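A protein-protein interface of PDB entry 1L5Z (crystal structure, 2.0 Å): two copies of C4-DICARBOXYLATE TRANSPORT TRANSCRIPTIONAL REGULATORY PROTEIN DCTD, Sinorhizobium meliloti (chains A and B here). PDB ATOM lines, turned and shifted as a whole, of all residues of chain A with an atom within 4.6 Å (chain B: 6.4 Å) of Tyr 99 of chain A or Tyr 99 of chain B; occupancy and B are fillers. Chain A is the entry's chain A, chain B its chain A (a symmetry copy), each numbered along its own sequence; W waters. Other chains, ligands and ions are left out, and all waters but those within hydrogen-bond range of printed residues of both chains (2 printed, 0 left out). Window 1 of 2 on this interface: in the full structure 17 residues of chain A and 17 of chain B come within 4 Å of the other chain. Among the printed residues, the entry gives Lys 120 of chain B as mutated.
The side-chain hydroxyl (OH) of Tyr 99 of chain B lies within hydrogen-bond range of the side-chain hydroxyl (OH) of Tyr 99 of chain A, 3.2 Å away. O of Tyr 99 of chain A sits at hydrogen-bond distance from NH1 of Arg 117 of chain B (2.8 Å). The side-chain carboxylate of Asp 100 of chain A is in salt-bridge range of the guanidinium group of Arg 117 of chain B (3.6 Å). The backbone carbonyl oxygen (O) of Tyr 99 of chain B is in hydrogen-bond range of the guanidinium group (NH1) of Arg 117 of chain A (2.8 Å). The side-chain carboxylate (OD1) of Asp 100 of chain B lies within salt-bridge range of the guanidinium group (NH1) of Arg 117 of chain A (3.6 Å).
O of Met 78 of chain A sits at hydrogen-bond distance from N of Tyr 99 of chain A (2.9 Å). The side-chain carboxylate (OD2) of Asp 100 of chain A is in salt-bridge range of the guanidinium group (NH2) of Arg 117 of chain A (3.2 Å). The backbone carbonyl oxygen (O) of Met 78 of chain B lies within hydrogen-bond range of the backbone NH (N) of Tyr 99 of chain B (2.8 Å). The backbone carbonyl oxygen of Asp 100 of chain B sits at hydrogen-bond distance from the backbone NH of Leu 80 of chain B. The side-chain carboxylate (OD2) of Asp 100 of chain B lies within hydrogen-bond range of the side-chain hydroxyl (OG) of Ser 114 of chain B (2.7 Å). The side-chain carboxylate of Asp 100 of chain B is in salt-bridge range of the guanidinium group of Arg 117 of chain B.
NE of Arg 117 of chain B touches NE of Arg 117 of chain A (3.8 Å).
Tyr 99 of chain A touches just these residues of chain B: Tyr 99 and Arg 117. Of chain A, only Tyr 99 and Arg 117 come within 4 Å of Tyr 99 of chain B. Printed residues of chain A within 4 Å of Asp 100 of chain B: Arg 117 (3.6 Å). Printed residues of chain A within 4 Å of Arg 117 of chain B: Tyr 99, Asp 100 and Arg 117. The nearest printed residue of chain A that does not touch Tyr 99 of chain B is Lys 121 of chain A (5.6 Å).
Of the 10 printed residues of chain A, 3 touch a printed residue of chain B. Hydrophobic or aromatic side chains of chain A that line the printed part of chain B: Tyr 99. Printed residues of chain B that touch a printed residue of chain A: Tyr 99, Asp 100 and Arg 117. Among the printed residues, 6 pairs touch across the chains.
Tyr 99 of chain A touches its own counterpart, Tyr 99 of chain B. Tyr 99 of chain A touches Arg 117 of chain B, and with the chains exchanged Arg 117 of chain A touches Tyr 99 of chain B. Asp 100 of chain A touches Arg 117 of chain B, and with the chains exchanged Arg 117 of chain A touches Asp 100 of chain B. Arg 117 of chain A touches its own counterpart, Arg 117 of chain B. 10 positions are printed for both chains. Of the 6 pairs that touch across the chains among the printed residues, 6 have their exchanged pair printed and touching as well.
Water W2 lies within hydrogen-bond range of the side-chain hydroxyl of Tyr 99 of chain A (2.6 Å), the backbone carbonyl oxygen of Arg 117 of chain B (2.9 Å) and the side-chain hydroxyl of Tyr 99 of chain B (3.4 Å). Water W1 lies within hydrogen-bond range of the side-chain hydroxyl (OH) of Tyr 99 of chain B (2.6 Å), the backbone carbonyl oxygen (O) of Arg 117 of chain A (2.9 Å) and the side-chain hydroxyl (OH) of Tyr 99 of chain A (3.4 Å).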
ATOM      1  N   PRO A  77       7.089  10.345   8.476  1.00  0.00           N
ATOM      2  CA  PRO A  77       6.651   9.433   7.427  1.00  0.00           C
ATOM      3  C   PRO A  77       5.447   8.560   7.660  1.00  0.00           C
ATOM      4  O   PRO A  77       5.222   7.991   8.737  1.00  0.00           O
ATOM      5  CB  PRO A  77       7.912   8.627   7.099  1.00  0.00           C
ATOM      6  CG  PRO A  77       8.660   8.620   8.341  1.00  0.00           C
ATOM      7  CD  PRO A  77       8.346   9.898   9.088  1.00  0.00           C
ATOM      8  N   MET A  78       4.673   8.474   6.597  1.00  0.00           N
ATOM      9  CA  MET A  78       3.466   7.685   6.610  1.00  0.00           C
ATOM     10  C   MET A  78       3.490   6.618   5.543  1.00  0.00           C
ATOM     11  O   MET A  78       3.747   6.914   4.346  1.00  0.00           O
ATOM     12  CB  MET A  78       2.225   8.537   6.432  1.00  0.00           C
ATOM     13  CG  MET A  78       0.997   7.748   6.863  1.00  0.00           C
ATOM     14  SD  MET A  78      -0.529   8.581   6.609  1.00  0.00           S
ATOM     15  CE  MET A  78      -1.715   7.183   6.554  1.00  0.00           C
ATOM     16  N   ILE A  94       2.040   9.277  -2.656  1.00  0.00           N
ATOM     17  CA  ILE A  94       3.479   9.395  -2.424  1.00  0.00           C
ATOM     18  C   ILE A  94       3.979  10.658  -3.146  1.00  0.00           C
ATOM     19  O   ILE A  94       4.724  11.446  -2.579  1.00  0.00           O
ATOM     20  CB  ILE A  94       4.236   8.093  -2.875  1.00  0.00           C
ATOM     21  CG1 ILE A  94       3.866   6.933  -1.922  1.00  0.00           C
ATOM     22  CG2 ILE A  94       5.811   8.311  -2.816  1.00  0.00           C
ATOM     23  CD1 ILE A  94       4.504   5.600  -2.333  1.00  0.00           C
ATOM     24  N   GLY A  97       3.595  13.485  -0.893  1.00  0.00           N
ATOM     25  CA  GLY A  97       4.175  13.560   0.443  1.00  0.00           C
ATOM     26  C   GLY A  97       4.113  12.313   1.305  1.00  0.00           C
ATOM     27  O   GLY A  97       4.780  12.267   2.343  1.00  0.00           O
ATOM     28  N   ALA A  98       3.319  11.316   0.903  1.00  0.00           N
ATOM     29  CA  ALA A  98       3.213  10.059   1.669  1.00  0.00           C
ATOM     30  C   ALA A  98       4.560   9.402   1.456  1.00  0.00           C
ATOM     31  O   ALA A  98       5.185   9.616   0.402  1.00  0.00           O
ATOM     32  CB  ALA A  98       2.097   9.186   1.133  1.00  0.00           C
ATOM     33  N   TYR A  99       5.004   8.602   2.424  1.00  0.00           N
ATOM     34  CA  TYR A  99       6.336   8.045   2.318  1.00  0.00           C
ATOM     35  C   TYR A  99       6.529   6.817   1.460  1.00  0.00           C
ATOM     36  O   TYR A  99       7.505   6.742   0.703  1.00  0.00           O
ATOM     37  CB  TYR A  99       6.897   7.753   3.705  1.00  0.00           C
ATOM     38  CG  TYR A  99       8.394   7.550   3.730  1.00  0.00           C
ATOM     39  CD1 TYR A  99       9.274   8.642   3.555  1.00  0.00           C
ATOM     40  CD2 TYR A  99       8.942   6.261   3.826  1.00  0.00           C
ATOM     41  CE1 TYR A  99      10.661   8.445   3.473  1.00  0.00           C
ATOM     42  CE2 TYR A  99      10.329   6.054   3.749  1.00  0.00           C
ATOM     43  CZ  TYR A  99      11.184   7.145   3.577  1.00  0.00           C
ATOM     44  OH  TYR A  99      12.557   6.937   3.562  1.00  0.00           O
ATOM     45  N   ASP A 100       5.592   5.879   1.547  1.00  0.00           N
ATOM     46  CA  ASP A 100       5.760   4.628   0.839  1.00  0.00           C
ATOM     47  C   ASP A 100       4.441   3.868   0.950  1.00  0.00           C
ATOM     48  O   ASP A 100       3.522   4.323   1.645  1.00  0.00           O
ATOM     49  CB  ASP A 100       6.876   3.868   1.570  1.00  0.00           C
ATOM     50  CG  ASP A 100       7.383   2.635   0.807  1.00  0.00           C
ATOM     51  OD1 ASP A 100       7.123   2.532  -0.405  1.00  0.00           O
ATOM     52  OD2 ASP A 100       8.055   1.794   1.450  1.00  0.00           O
ATOM     53  N   ARG A 117      13.092   1.502   6.732  1.00  0.00           N
ATOM     54  CA  ARG A 117      13.572   2.629   5.921  1.00  0.00           C
ATOM     55  C   ARG A 117      12.912   3.927   6.401  1.00  0.00           C
ATOM     56  O   ARG A 117      13.589   4.941   6.569  1.00  0.00           O
ATOM     57  CB  ARG A 117      13.247   2.388   4.440  1.00  0.00           C
ATOM     58  CG  ARG A 117      13.772   3.461   3.483  1.00  0.00           C
ATOM     59  CD  ARG A 117      13.782   2.909   2.013  1.00  0.00           C
ATOM     60  NE  ARG A 117      12.478   2.373   1.659  1.00  0.00           N
ATOM     61  CZ  ARG A 117      12.252   1.169   1.134  1.00  0.00           C
ATOM     62  NH1 ARG A 117      13.244   0.332   0.867  1.00  0.00           N
ATOM     63  NH2 ARG A 117      10.998   0.784   0.925  1.00  0.00           N
ATOM     64  N   ALA A 118      11.591   3.883   6.623  1.00  0.00           N
ATOM     65  CA  ALA A 118      10.863   5.048   7.080  1.00  0.00           C
ATOM     66  C   ALA A 118      11.346   5.502   8.462  1.00  0.00           C
ATOM     67  O   ALA A 118      11.476   6.705   8.712  1.00  0.00           O
ATOM     68  CB  ALA A 118       9.380   4.758   7.133  1.00  0.00           C
ATOM     69  N   LYS A 121      14.599   7.271   8.275  1.00  0.00           N
ATOM     70  CA  LYS A 121      14.372   8.623   7.777  1.00  0.00           C
ATOM     71  C   LYS A 121      13.938   9.502   8.948  1.00  0.00           C
ATOM     72  O   LYS A 121      14.497  10.568   9.174  1.00  0.00           O
ATOM     73  CB  LYS A 121      13.267   8.646   6.692  1.00  0.00           C
ATOM     74  CG  LYS A 121      13.010  10.027   6.079  1.00  0.00           C
ATOM     75  CD  LYS A 121      11.999  10.849   6.925  1.00  0.00           C
ATOM     76  CE  LYS A 121      11.568  12.192   6.249  1.00  0.00           C
ATOM     77  NZ  LYS A 121      10.476  12.064   5.245  1.00  0.00           N
ATOM     78  N   PHE B  66      27.054  -3.337  -5.317  1.00  0.00           N
ATOM     79  CA  PHE B  66      26.516  -3.039  -3.995  1.00  0.00           C
ATOM     80  C   PHE B  66      27.523  -3.375  -2.856  1.00  0.00           C
ATOM     81  O   PHE B  66      27.748  -2.558  -1.964  1.00  0.00           O
ATOM     82  CB  PHE B  66      25.218  -3.807  -3.731  1.00  0.00           C
ATOM     83  CG  PHE B  66      24.798  -3.774  -2.278  1.00  0.00           C
ATOM     84  CD1 PHE B  66      24.494  -2.556  -1.654  1.00  0.00           C
ATOM     85  CD2 PHE B  66      24.774  -4.948  -1.511  1.00  0.00           C
ATOM     86  CE1 PHE B  66      24.169  -2.489  -0.276  1.00  0.00           C
ATOM     87  CE2 PHE B  66      24.453  -4.899  -0.134  1.00  0.00           C
ATOM     88  CZ  PHE B  66      24.151  -3.662   0.488  1.00  0.00           C
ATOM     89  N   LEU B  76      25.384   5.332   1.849  1.00  0.00           N
ATOM     90  CA  LEU B  76      25.334   5.841   0.473  1.00  0.00           C
ATOM     91  C   LEU B  76      24.264   4.896  -0.130  1.00  0.00           C
ATOM     92  O   LEU B  76      24.545   3.740  -0.461  1.00  0.00           O
ATOM     93  CB  LEU B  76      26.709   5.646  -0.193  1.00  0.00           C
ATOM     94  CG  LEU B  76      27.022   6.542  -1.408  1.00  0.00           C
ATOM     95  CD1 LEU B  76      28.401   6.218  -2.002  1.00  0.00           C
ATOM     96  CD2 LEU B  76      25.944   6.340  -2.438  1.00  0.00           C
ATOM     97  N   PRO B  77      23.026   5.376  -0.280  1.00  0.00           N
ATOM     98  CA  PRO B  77      22.024   4.463  -0.816  1.00  0.00           C
ATOM     99  C   PRO B  77      22.152   3.973  -2.234  1.00  0.00           C
ATOM    100  O   PRO B  77      22.503   4.701  -3.172  1.00  0.00           O
ATOM    101  CB  PRO B  77      20.700   5.188  -0.558  1.00  0.00           C
ATOM    102  CG  PRO B  77      21.055   6.594  -0.585  1.00  0.00           C
ATOM    103  CD  PRO B  77      22.484   6.728  -0.105  1.00  0.00           C
ATOM    104  N   MET B  78      21.851   2.696  -2.355  1.00  0.00           N
ATOM    105  CA  MET B  78      21.909   2.030  -3.632  1.00  0.00           C
ATOM    106  C   MET B  78      20.574   1.436  -4.010  1.00  0.00           C
ATOM    107  O   MET B  78      19.957   0.684  -3.208  1.00  0.00           O
ATOM    108  CB  MET B  78      22.962   0.940  -3.661  1.00  0.00           C
ATOM    109  CG  MET B  78      23.273   0.566  -5.103  1.00  0.00           C
ATOM    110  SD  MET B  78      24.405  -0.765  -5.282  1.00  0.00           S
ATOM    111  CE  MET B  78      24.011  -1.370  -6.967  1.00  0.00           C
ATOM    112  N   ILE B  79      20.096   1.806  -5.199  1.00  0.00           N
ATOM    113  CA  ILE B  79      18.841   1.267  -5.724  1.00  0.00           C
ATOM    114  C   ILE B  79      19.089   0.243  -6.864  1.00  0.00           C
ATOM    115  O   ILE B  79      19.827   0.502  -7.838  1.00  0.00           O
ATOM    116  CB  ILE B  79      17.898   2.388  -6.236  1.00  0.00           C
ATOM    117  CG1 ILE B  79      17.590   3.377  -5.094  1.00  0.00           C
ATOM    118  CG2 ILE B  79      16.596   1.764  -6.787  1.00  0.00           C
ATOM    119  CD1 ILE B  79      16.753   4.577  -5.519  1.00  0.00           C
ATOM    120  N   LEU B  80      18.471  -0.923  -6.726  1.00  0.00           N
ATOM    121  CA  LEU B  80      18.607  -1.984  -7.720  1.00  0.00           C
ATOM    122  C   LEU B  80      17.434  -2.031  -8.694  1.00  0.00           C
ATOM    123  O   LEU B  80      16.271  -2.088  -8.265  1.00  0.00           O
ATOM    124  CB  LEU B  80      18.717  -3.327  -7.009  1.00  0.00           C
ATOM    125  CG  LEU B  80      19.953  -3.450  -6.109  1.00  0.00           C
ATOM    126  CD1 LEU B  80      19.724  -4.601  -5.114  1.00  0.00           C
ATOM    127  CD2 LEU B  80      21.197  -3.690  -6.977  1.00  0.00           C
ATOM    128  N   ALA B  93      18.940  -8.458  -0.778  1.00  0.00           N
ATOM    129  CA  ALA B  93      19.998  -7.464  -0.763  1.00  0.00           C
ATOM    130  C   ALA B  93      19.586  -6.297   0.130  1.00  0.00           C
ATOM    131  O   ALA B  93      20.422  -5.716   0.831  1.00  0.00           O
ATOM    132  CB  ALA B  93      20.323  -6.961  -2.201  1.00  0.00           C
ATOM    133  N   ILE B  94      18.300  -5.942   0.089  1.00  0.00           N
ATOM    134  CA  ILE B  94      17.827  -4.836   0.921  1.00  0.00           C
ATOM    135  C   ILE B  94      18.011  -5.233   2.396  1.00  0.00           C
ATOM    136  O   ILE B  94      18.506  -4.448   3.195  1.00  0.00           O
ATOM    137  CB  ILE B  94      16.342  -4.456   0.571  1.00  0.00           C
ATOM    138  CG1 ILE B  94      16.298  -3.821  -0.839  1.00  0.00           C
ATOM    139  CG2 ILE B  94      15.771  -3.402   1.617  1.00  0.00           C
ATOM    140  CD1 ILE B  94      14.873  -3.486  -1.295  1.00  0.00           C
ATOM    141  N   GLY B  97      21.369  -4.290   3.419  1.00  0.00           N
ATOM    142  CA  GLY B  97      21.914  -2.941   3.321  1.00  0.00           C
ATOM    143  C   GLY B  97      21.613  -2.154   2.058  1.00  0.00           C
ATOM    144  O   GLY B  97      21.863  -0.945   2.031  1.00  0.00           O
ATOM    145  N   ALA B  98      21.097  -2.815   1.019  1.00  0.00           N
ATOM    146  CA  ALA B  98      20.756  -2.127  -0.241  1.00  0.00           C
ATOM    147  C   ALA B  98      19.555  -1.284   0.134  1.00  0.00           C
ATOM    148  O   ALA B  98      18.792  -1.673   1.036  1.00  0.00           O
ATOM    149  CB  ALA B  98      20.397  -3.120  -1.327  1.00  0.00           C
ATOM    150  N   TYR B  99      19.371  -0.154  -0.548  1.00  0.00           N
ATOM    151  CA  TYR B  99      18.306   0.741  -0.148  1.00  0.00           C
ATOM    152  C   TYR B  99      16.904   0.437  -0.621  1.00  0.00           C
ATOM    153  O   TYR B  99      15.953   0.543   0.163  1.00  0.00           O
ATOM    154  CB  TYR B  99      18.644   2.173  -0.544  1.00  0.00           C
ATOM    155  CG  TYR B  99      17.812   3.217   0.163  1.00  0.00           C
ATOM    156  CD1 TYR B  99      18.017   3.500   1.532  1.00  0.00           C
ATOM    157  CD2 TYR B  99      16.750   3.856  -0.499  1.00  0.00           C
ATOM    158  CE1 TYR B  99      17.178   4.392   2.218  1.00  0.00           C
ATOM    159  CE2 TYR B  99      15.908   4.754   0.178  1.00  0.00           C
ATOM    160  CZ  TYR B  99      16.127   5.022   1.531  1.00  0.00           C
ATOM    161  OH  TYR B  99      15.326   5.956   2.176  1.00  0.00           O
ATOM    162  N   ASP B 100      16.777   0.028  -1.878  1.00  0.00           N
ATOM    163  CA  ASP B 100      15.459  -0.179  -2.438  1.00  0.00           C
ATOM    164  C   ASP B 100      15.646  -0.853  -3.795  1.00  0.00           C
ATOM    165  O   ASP B 100      16.787  -1.027  -4.245  1.00  0.00           O
ATOM    166  CB  ASP B 100      14.844   1.217  -2.616  1.00  0.00           C
ATOM    167  CG  ASP B 100      13.344   1.191  -2.946  1.00  0.00           C
ATOM    168  OD1 ASP B 100      12.701   0.150  -2.730  1.00  0.00           O
ATOM    169  OD2 ASP B 100      12.837   2.242  -3.408  1.00  0.00           O
ATOM    170  N   PHE B 101      14.543  -1.265  -4.409  1.00  0.00           N
ATOM    171  CA  PHE B 101      14.582  -1.857  -5.755  1.00  0.00           C
ATOM    172  C   PHE B 101      13.402  -1.328  -6.556  1.00  0.00           C
ATOM    173  O   PHE B 101      12.390  -0.878  -5.996  1.00  0.00           O
ATOM    174  CB  PHE B 101      14.566  -3.415  -5.756  1.00  0.00           C
ATOM    175  CG  PHE B 101      13.213  -4.024  -5.558  1.00  0.00           C
ATOM    176  CD1 PHE B 101      12.333  -4.172  -6.627  1.00  0.00           C
ATOM    177  CD2 PHE B 101      12.808  -4.438  -4.290  1.00  0.00           C
ATOM    178  CE1 PHE B 101      11.054  -4.729  -6.450  1.00  0.00           C
ATOM    179  CE2 PHE B 101      11.530  -4.999  -4.084  1.00  0.00           C
ATOM    180  CZ  PHE B 101      10.646  -5.146  -5.171  1.00  0.00           C
ATOM    181  N   SER B 114      11.327   6.540  -5.992  1.00  0.00           N
ATOM    182  CA  SER B 114      12.363   5.774  -5.301  1.00  0.00           C
ATOM    183  C   SER B 114      13.658   6.615  -5.226  1.00  0.00           C
ATOM    184  O   SER B 114      14.291   6.704  -4.172  1.00  0.00           O
ATOM    185  CB  SER B 114      12.587   4.443  -6.048  1.00  0.00           C
ATOM    186  OG  SER B 114      13.633   3.687  -5.497  1.00  0.00           O
ATOM    187  N   ARG B 117      13.292   9.492  -2.644  1.00  0.00           N
ATOM    188  CA  ARG B 117      13.344   9.038  -1.248  1.00  0.00           C
ATOM    189  C   ARG B 117      14.796   8.745  -0.854  1.00  0.00           C
ATOM    190  O   ARG B 117      15.244   9.155   0.216  1.00  0.00           O
ATOM    191  CB  ARG B 117      12.484   7.778  -1.070  1.00  0.00           C
ATOM    192  CG  ARG B 117      12.394   7.257   0.366  1.00  0.00           C
ATOM    193  CD  ARG B 117      11.175   6.277   0.504  1.00  0.00           C
ATOM    194  NE  ARG B 117      11.236   5.238  -0.510  1.00  0.00           N
ATOM    195  CZ  ARG B 117      10.242   4.896  -1.328  1.00  0.00           C
ATOM    196  NH1 ARG B 117       9.060   5.491  -1.271  1.00  0.00           N
ATOM    197  NH2 ARG B 117      10.463   3.971  -2.257  1.00  0.00           N
ATOM    198  N   ALA B 118      15.524   8.037  -1.730  1.00  0.00           N
ATOM    199  CA  ALA B 118      16.908   7.703  -1.465  1.00  0.00           C
ATOM    200  C   ALA B 118      17.776   8.961  -1.358  1.00  0.00           C
ATOM    201  O   ALA B 118      18.658   9.039  -0.495  1.00  0.00           O
ATOM    202  CB  ALA B 118      17.452   6.802  -2.552  1.00  0.00           C
ATOM    203  N   GLU B 119      17.526   9.931  -2.246  1.00  0.00           N
ATOM    204  CA  GLU B 119      18.289  11.165  -2.237  1.00  0.00           C
ATOM    205  C   GLU B 119      17.994  11.998  -0.974  1.00  0.00           C
ATOM    206  O   GLU B 119      18.883  12.650  -0.442  1.00  0.00           O
ATOM    207  CB  GLU B 119      17.992  11.959  -3.507  1.00  0.00           C
ATOM    208  CG  GLU B 119      18.967  13.072  -3.796  1.00  0.00           C
ATOM    209  CD  GLU B 119      18.749  14.284  -2.907  1.00  0.00           C
ATOM    210  OE1 GLU B 119      17.575  14.575  -2.565  1.00  0.00           O
ATOM    211  OE2 GLU B 119      19.762  14.950  -2.563  1.00  0.00           O
ATOM    212  N   LYS B 120      16.758  11.985  -0.491  1.00  0.00           N
ATOM    213  CA  LYS B 120      16.460  12.701   0.750  1.00  0.00           C
ATOM    214  C   LYS B 120      17.228  12.036   1.888  1.00  0.00           C
ATOM    215  O   LYS B 120      17.729  12.710   2.772  1.00  0.00           O
ATOM    216  CB  LYS B 120      14.957  12.645   1.088  1.00  0.00           C
ATOM    217  CG  LYS B 120      14.043  13.221   0.033  1.00  0.00           C
ATOM    218  CD  LYS B 120      14.146  14.724  -0.061  1.00  0.00           C
ATOM    219  CE  LYS B 120      12.888  15.308  -0.715  1.00  0.00           C
ATOM    220  NZ  LYS B 120      12.903  16.809  -0.656  1.00  0.00           N
ATOM    221  N   LYS B 121      17.294  10.702   1.880  1.00  0.00           N
ATOM    222  CA  LYS B 121      18.013   9.973   2.918  1.00  0.00           C
ATOM    223  C   LYS B 121      19.477  10.400   2.883  1.00  0.00           C
ATOM    224  O   LYS B 121      20.050  10.767   3.902  1.00  0.00           O
ATOM    225  CB  LYS B 121      17.928   8.443   2.693  1.00  0.00           C
ATOM    226  CG  LYS B 121      18.613   7.604   3.778  1.00  0.00           C
ATOM    227  CD  LYS B 121      20.128   7.420   3.487  1.00  0.00           C
ATOM    228  CE  LYS B 121      20.835   6.427   4.466  1.00  0.00           C
ATOM    229  NZ  LYS B 121      20.691   4.989   4.109  1.00  0.00           N
HETATM  230  O   HOH W   1      15.605   6.070   4.756  1.00  0.00           O
HETATM  231  O   HOH W   2      13.988   8.989   2.865  1.00  0.00           O
